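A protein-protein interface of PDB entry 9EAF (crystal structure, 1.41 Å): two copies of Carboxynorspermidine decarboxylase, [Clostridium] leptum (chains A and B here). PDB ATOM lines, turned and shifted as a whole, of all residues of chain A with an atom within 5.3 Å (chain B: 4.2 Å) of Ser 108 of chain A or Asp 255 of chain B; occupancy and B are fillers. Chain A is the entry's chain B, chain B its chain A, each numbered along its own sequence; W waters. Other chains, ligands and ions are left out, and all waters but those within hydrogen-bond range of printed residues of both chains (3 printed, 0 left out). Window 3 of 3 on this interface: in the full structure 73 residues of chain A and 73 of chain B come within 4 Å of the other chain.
The side-chain carboxylate (OD2) of Asp 255 of chain B sits at hydrogen-bond distance from the side-chain hydroxyl (OG) of Ser 106 of chain A (3.0 Å). OG of Ser 108 of chain A is in hydrogen-bond range of OD1 of Asp 255 of chain B.
The backbone NH (N) of Leu 254 of chain B sits at hydrogen-bond distance from the backbone carbonyl oxygen (O) of Val 265 of chain B (2.8 Å). N of Val 265 of chain B lies within hydrogen-bond range of O of Asp 255 of chain B. The side-chain hydroxyl (OG) of Ser 106 of chain A lies within hydrogen-bond range of the side-chain hydroxyl (OG) of Ser 108 of chain A, 2.9 Å away. OG of Ser 106 of chain A is in hydrogen-bond range of N of Gln 109 of chain A (3.1 Å).
Among the printed residues, merely in contact across the chains: Ala 86 of chain A with Leu 254 of chain B, Ala 86 of chain A with Val 265 of chain B and Gln 109 of chain A with Asp 255 of chain B.
Printed residues of chain B within 4 Å of Ser 108 of chain A: Asp 255 (2.9 Å). Of the printed residues of chain B, Gln 109 of chain A touches Asp 255. Of the printed residues of chain A, Leu 254 of chain B touches Ala 86. Printed residues of chain A within 4 Å of Val 265 of chain B: Ala 86 (3.9 Å). The nearest printed residue of chain B that does not touch Ser 108 of chain A is Val 256 of chain B (4.8 Å). The nearest printed residue of chain B that does not touch Ala 86 of chain A is Asp 255 of chain B (4.05 Å).
Of the 10 printed residues of chain A, 4 touch a printed residue of chain B. Hydrophobic or aromatic side chains of chain B within 4 Å of the printed part of chain A: Leu 254 and Val 265. Among the printed residues, no Asp or Glu carboxylate lies within 4 Å of a Lys or Arg side-chain nitrogen of the other chain.
No position is printed for both chains.
Water W2 bridges the backbone carbonyl oxygen (O) of Pro 85 of chain A (2.6 Å) and the side-chain carboxylate (OD2) of Asp 255 of chain B (2.6 Å). Water W3 lies within hydrogen-bond range of OG of Ser 108 of chain A (2.6 Å), O of Val 256 of chain B (2.8 Å) and OD1 of Asp 255 of chain B (3.4 Å). Water W1 lies within hydrogen-bond range of the side-chain carboxylate of Asp 255 of chain B (2.8 Å) and the side-chain amide nitrogen of Gln 109 of chain A (2.9 Å).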
ATOM      1  N   PRO A  85     -13.466   1.745 -20.101  1.00  0.00           N
ATOM      2  CA  PRO A  85     -12.898   1.324 -18.810  1.00  0.00           C
ATOM      3  C   PRO A  85     -12.543   2.493 -17.914  1.00  0.00           C
ATOM      4  O   PRO A  85     -12.605   2.368 -16.685  1.00  0.00           O
ATOM      5  CB  PRO A  85     -11.653   0.522 -19.219  1.00  0.00           C
ATOM      6  CG  PRO A  85     -11.970   0.029 -20.587  1.00  0.00           C
ATOM      7  CD  PRO A  85     -12.755   1.130 -21.237  1.00  0.00           C
ATOM      8  N   ALA A  86     -12.166   3.629 -18.496  1.00  0.00           N
ATOM      9  CA  ALA A  86     -11.907   4.833 -17.714  1.00  0.00           C
ATOM     10  C   ALA A  86     -11.989   6.032 -18.640  1.00  0.00           C
ATOM     11  O   ALA A  86     -11.246   6.110 -19.623  1.00  0.00           O
ATOM     12  CB  ALA A  86     -10.534   4.767 -17.044  1.00  0.00           C
ATOM     13  N   SER A 106     -16.642   1.190 -13.130  1.00  0.00           N
ATOM     14  CA  SER A 106     -16.355   0.977 -11.722  1.00  0.00           C
ATOM     15  C   SER A 106     -17.130   2.006 -10.918  1.00  0.00           C
ATOM     16  O   SER A 106     -17.587   3.019 -11.451  1.00  0.00           O
ATOM     17  CB  SER A 106     -14.861   1.134 -11.433  1.00  0.00           C
ATOM     18  OG  SER A 106     -14.458   2.472 -11.652  1.00  0.00           O
ATOM     19  N   PHE A 107     -17.259   1.741  -9.617  1.00  0.00           N
ATOM     20  CA  PHE A 107     -17.924   2.707  -8.752  1.00  0.00           C
ATOM     21  C   PHE A 107     -17.082   3.960  -8.560  1.00  0.00           C
ATOM     22  O   PHE A 107     -17.635   5.054  -8.406  1.00  0.00           O
ATOM     23  CB  PHE A 107     -18.336   2.055  -7.431  1.00  0.00           C
ATOM     24  CG  PHE A 107     -19.621   1.287  -7.535  1.00  0.00           C
ATOM     25  CD1 PHE A 107     -20.838   1.936  -7.425  1.00  0.00           C
ATOM     26  CD2 PHE A 107     -19.614  -0.075  -7.795  1.00  0.00           C
ATOM     27  CE1 PHE A 107     -22.028   1.239  -7.544  1.00  0.00           C
ATOM     28  CE2 PHE A 107     -20.800  -0.778  -7.914  1.00  0.00           C
ATOM     29  CZ  PHE A 107     -22.008  -0.121  -7.790  1.00  0.00           C
ATOM     30  N   SER A 108     -15.753   3.839  -8.597  1.00  0.00           N
ATOM     31  CA  SER A 108     -14.918   5.034  -8.542  1.00  0.00           C
ATOM     32  C   SER A 108     -15.179   5.933  -9.747  1.00  0.00           C
ATOM     33  O   SER A 108     -15.285   7.156  -9.608  1.00  0.00           O
ATOM     34  CB  SER A 108     -13.439   4.650  -8.446  1.00  0.00           C
ATOM     35  OG  SER A 108     -12.998   3.948  -9.596  1.00  0.00           O
ATOM     36  N   GLN A 109     -15.300   5.343 -10.935  1.00  0.00           N
ATOM     37  CA  GLN A 109     -15.607   6.135 -12.120  1.00  0.00           C
ATOM     38  C   GLN A 109     -16.982   6.784 -12.012  1.00  0.00           C
ATOM     39  O   GLN A 109     -17.146   7.970 -12.317  1.00  0.00           O
ATOM     40  CB  GLN A 109     -15.529   5.240 -13.353  1.00  0.00           C
ATOM     41  CG  GLN A 109     -14.106   4.985 -13.804  1.00  0.00           C
ATOM     42  CD  GLN A 109     -13.594   6.094 -14.685  1.00  0.00           C
ATOM     43  OE1 GLN A 109     -14.131   6.327 -15.772  1.00  0.00           O
ATOM     44  NE2 GLN A 109     -12.569   6.801 -14.221  1.00  0.00           N
ATOM     45  N   TRP A 110     -17.986   6.017 -11.589  1.00  0.00           N
ATOM     46  CA  TRP A 110     -19.333   6.565 -11.452  1.00  0.00           C
ATOM     47  C   TRP A 110     -19.353   7.733 -10.474  1.00  0.00           C
ATOM     48  O   TRP A 110     -19.892   8.803 -10.775  1.00  0.00           O
ATOM     49  CB  TRP A 110     -20.283   5.450 -11.011  1.00  0.00           C
ATOM     50  CG  TRP A 110     -21.637   5.875 -10.498  1.00  0.00           C
ATOM     51  CD1 TRP A 110     -22.216   5.483  -9.328  1.00  0.00           C
ATOM     52  CD2 TRP A 110     -22.582   6.748 -11.137  1.00  0.00           C
ATOM     53  NE1 TRP A 110     -23.458   6.048  -9.197  1.00  0.00           N
ATOM     54  CE2 TRP A 110     -23.707   6.833 -10.290  1.00  0.00           C
ATOM     55  CE3 TRP A 110     -22.587   7.464 -12.336  1.00  0.00           C
ATOM     56  CZ2 TRP A 110     -24.827   7.604 -10.605  1.00  0.00           C
ATOM     57  CZ3 TRP A 110     -23.698   8.230 -12.648  1.00  0.00           C
ATOM     58  CH2 TRP A 110     -24.803   8.293 -11.785  1.00  0.00           C
ATOM     59  N   GLU A 111     -18.754   7.555  -9.298  1.00  0.00           N
ATOM     60  CA  GLU A 111     -18.798   8.619  -8.300  1.00  0.00           C
ATOM     61  C   GLU A 111     -18.028   9.850  -8.760  1.00  0.00           C
ATOM     62  O   GLU A 111     -18.405  10.978  -8.423  1.00  0.00           O
ATOM     63  CB  GLU A 111     -18.258   8.110  -6.964  1.00  0.00           C
ATOM     64  CG  GLU A 111     -19.119   7.028  -6.324  1.00  0.00           C
ATOM     65  CD  GLU A 111     -20.525   7.506  -5.986  1.00  0.00           C
ATOM     66  OE1 GLU A 111     -20.698   8.709  -5.697  1.00  0.00           O
ATOM     67  OE2 GLU A 111     -21.459   6.680  -6.008  1.00  0.00           O
ATOM     68  N   LYS A 112     -16.960   9.656  -9.534  1.00  0.00           N
ATOM     69  CA  LYS A 112     -16.186  10.788 -10.030  1.00  0.00           C
ATOM     70  C   LYS A 112     -17.025  11.673 -10.941  1.00  0.00           C
ATOM     71  O   LYS A 112     -16.948  12.904 -10.866  1.00  0.00           O
ATOM     72  CB  LYS A 112     -14.951  10.270 -10.772  1.00  0.00           C
ATOM     73  CG  LYS A 112     -14.052  11.349 -11.347  1.00  0.00           C
ATOM     74  CD  LYS A 112     -12.842  10.737 -12.041  1.00  0.00           C
ATOM     75  CE  LYS A 112     -11.944  11.799 -12.647  1.00  0.00           C
ATOM     76  NZ  LYS A 112     -11.164  12.533 -11.614  1.00  0.00           N
ATOM     77  N   TYR A 113     -17.840  11.065 -11.806  1.00  0.00           N
ATOM     78  CA  TYR A 113     -18.566  11.793 -12.838  1.00  0.00           C
ATOM     79  C   TYR A 113     -20.055  11.934 -12.553  1.00  0.00           C
ATOM     80  O   TYR A 113     -20.768  12.539 -13.360  1.00  0.00           O
ATOM     81  CB  TYR A 113     -18.334  11.123 -14.199  1.00  0.00           C
ATOM     82  CG  TYR A 113     -16.882  11.168 -14.613  1.00  0.00           C
ATOM     83  CD1 TYR A 113     -16.235  12.382 -14.780  1.00  0.00           C
ATOM     84  CD2 TYR A 113     -16.153  10.004 -14.815  1.00  0.00           C
ATOM     85  CE1 TYR A 113     -14.910  12.442 -15.150  1.00  0.00           C
ATOM     86  CE2 TYR A 113     -14.817  10.053 -15.187  1.00  0.00           C
ATOM     87  CZ  TYR A 113     -14.205  11.278 -15.352  1.00  0.00           C
ATOM     88  OH  TYR A 113     -12.880  11.350 -15.718  1.00  0.00           O
ATOM     89  N   VAL B 253      -2.045   7.033 -15.417  1.00  0.00           N
ATOM     90  CA  VAL B 253      -3.020   6.097 -14.871  1.00  0.00           C
ATOM     91  C   VAL B 253      -4.367   6.793 -14.753  1.00  0.00           C
ATOM     92  O   VAL B 253      -4.477   7.875 -14.158  1.00  0.00           O
ATOM     93  CB  VAL B 253      -2.562   5.592 -13.494  1.00  0.00           C
ATOM     94  CG1 VAL B 253      -3.639   4.711 -12.873  1.00  0.00           C
ATOM     95  CG2 VAL B 253      -1.245   4.841 -13.594  1.00  0.00           C
ATOM     96  N   LEU B 254      -5.405   6.169 -15.302  1.00  0.00           N
ATOM     97  CA  LEU B 254      -6.758   6.716 -15.248  1.00  0.00           C
ATOM     98  C   LEU B 254      -7.592   6.159 -14.104  1.00  0.00           C
ATOM     99  O   LEU B 254      -8.408   6.887 -13.523  1.00  0.00           O
ATOM    100  CB  LEU B 254      -7.488   6.442 -16.564  1.00  0.00           C
ATOM    101  CG  LEU B 254      -6.899   7.099 -17.810  1.00  0.00           C
ATOM    102  CD1 LEU B 254      -7.655   6.667 -19.053  1.00  0.00           C
ATOM    103  CD2 LEU B 254      -6.916   8.613 -17.664  1.00  0.00           C
ATOM    104  N   ASP B 255      -7.436   4.880 -13.782  1.00  0.00           N
ATOM    105  CA  ASP B 255      -8.214   4.264 -12.715  1.00  0.00           C
ATOM    106  C   ASP B 255      -7.417   3.080 -12.197  1.00  0.00           C
ATOM    107  O   ASP B 255      -6.587   2.514 -12.918  1.00  0.00           O
ATOM    108  CB  ASP B 255      -9.586   3.799 -13.229  1.00  0.00           C
ATOM    109  CG  ASP B 255     -10.600   3.554 -12.110  1.00  0.00           C
ATOM    110  OD1 ASP B 255     -10.431   4.090 -10.998  1.00  0.00           O
ATOM    111  OD2 ASP B 255     -11.585   2.824 -12.356  1.00  0.00           O
ATOM    112  N   VAL B 256      -7.654   2.731 -10.936  1.00  0.00           N
ATOM    113  CA  VAL B 256      -7.093   1.533 -10.326  1.00  0.00           C
ATOM    114  C   VAL B 256      -8.230   0.788  -9.644  1.00  0.00           C
ATOM    115  O   VAL B 256      -9.025   1.393  -8.917  1.00  0.00           O
ATOM    116  CB  VAL B 256      -5.973   1.865  -9.321  1.00  0.00           C
ATOM    117  CG1 VAL B 256      -5.451   0.594  -8.661  1.00  0.00           C
ATOM    118  CG2 VAL B 256      -4.833   2.596 -10.016  1.00  0.00           C
ATOM    119  N   ILE B 263      -5.245  -3.784 -10.426  1.00  0.00           N
ATOM    120  CA  ILE B 263      -5.354  -3.553 -11.861  1.00  0.00           C
ATOM    121  C   ILE B 263      -5.318  -2.048 -12.089  1.00  0.00           C
ATOM    122  O   ILE B 263      -6.034  -1.298 -11.417  1.00  0.00           O
ATOM    123  CB  ILE B 263      -6.660  -4.141 -12.429  1.00  0.00           C
ATOM    124  CG1 ILE B 263      -6.898  -5.602 -12.000  1.00  0.00           C
ATOM    125  CG2 ILE B 263      -6.683  -4.008 -13.939  1.00  0.00           C
ATOM    126  CD1 ILE B 263      -5.673  -6.492 -11.865  1.00  0.00           C
ATOM    127  N   ALA B 264      -4.493  -1.606 -13.033  1.00  0.00           N
ATOM    128  CA  ALA B 264      -4.403  -0.197 -13.394  1.00  0.00           C
ATOM    129  C   ALA B 264      -4.801  -0.025 -14.851  1.00  0.00           C
ATOM    130  O   ALA B 264      -4.264  -0.707 -15.730  1.00  0.00           O
ATOM    131  CB  ALA B 264      -2.983   0.334 -13.184  1.00  0.00           C
ATOM    132  N   VAL B 265      -5.746   0.880 -15.100  1.00  0.00           N
ATOM    133  CA  VAL B 265      -6.136   1.256 -16.454  1.00  0.00           C
ATOM    134  C   VAL B 265      -5.345   2.500 -16.841  1.00  0.00           C
ATOM    135  O   VAL B 265      -5.489   3.555 -16.213  1.00  0.00           O
ATOM    136  CB  VAL B 265      -7.646   1.526 -16.540  1.00  0.00           C
ATOM    137  CG1 VAL B 265      -8.032   1.954 -17.951  1.00  0.00           C
ATOM    138  CG2 VAL B 265      -8.443   0.306 -16.097  1.00  0.00           C
HETATM  139  O   HOH W   1     -11.559   6.634 -11.548  1.00  0.00           O
HETATM  140  O   HOH W   2     -12.193   1.289 -14.393  1.00  0.00           O
HETATM  141  O   HOH W   3     -11.751   1.794  -8.862  1.00  0.00           O
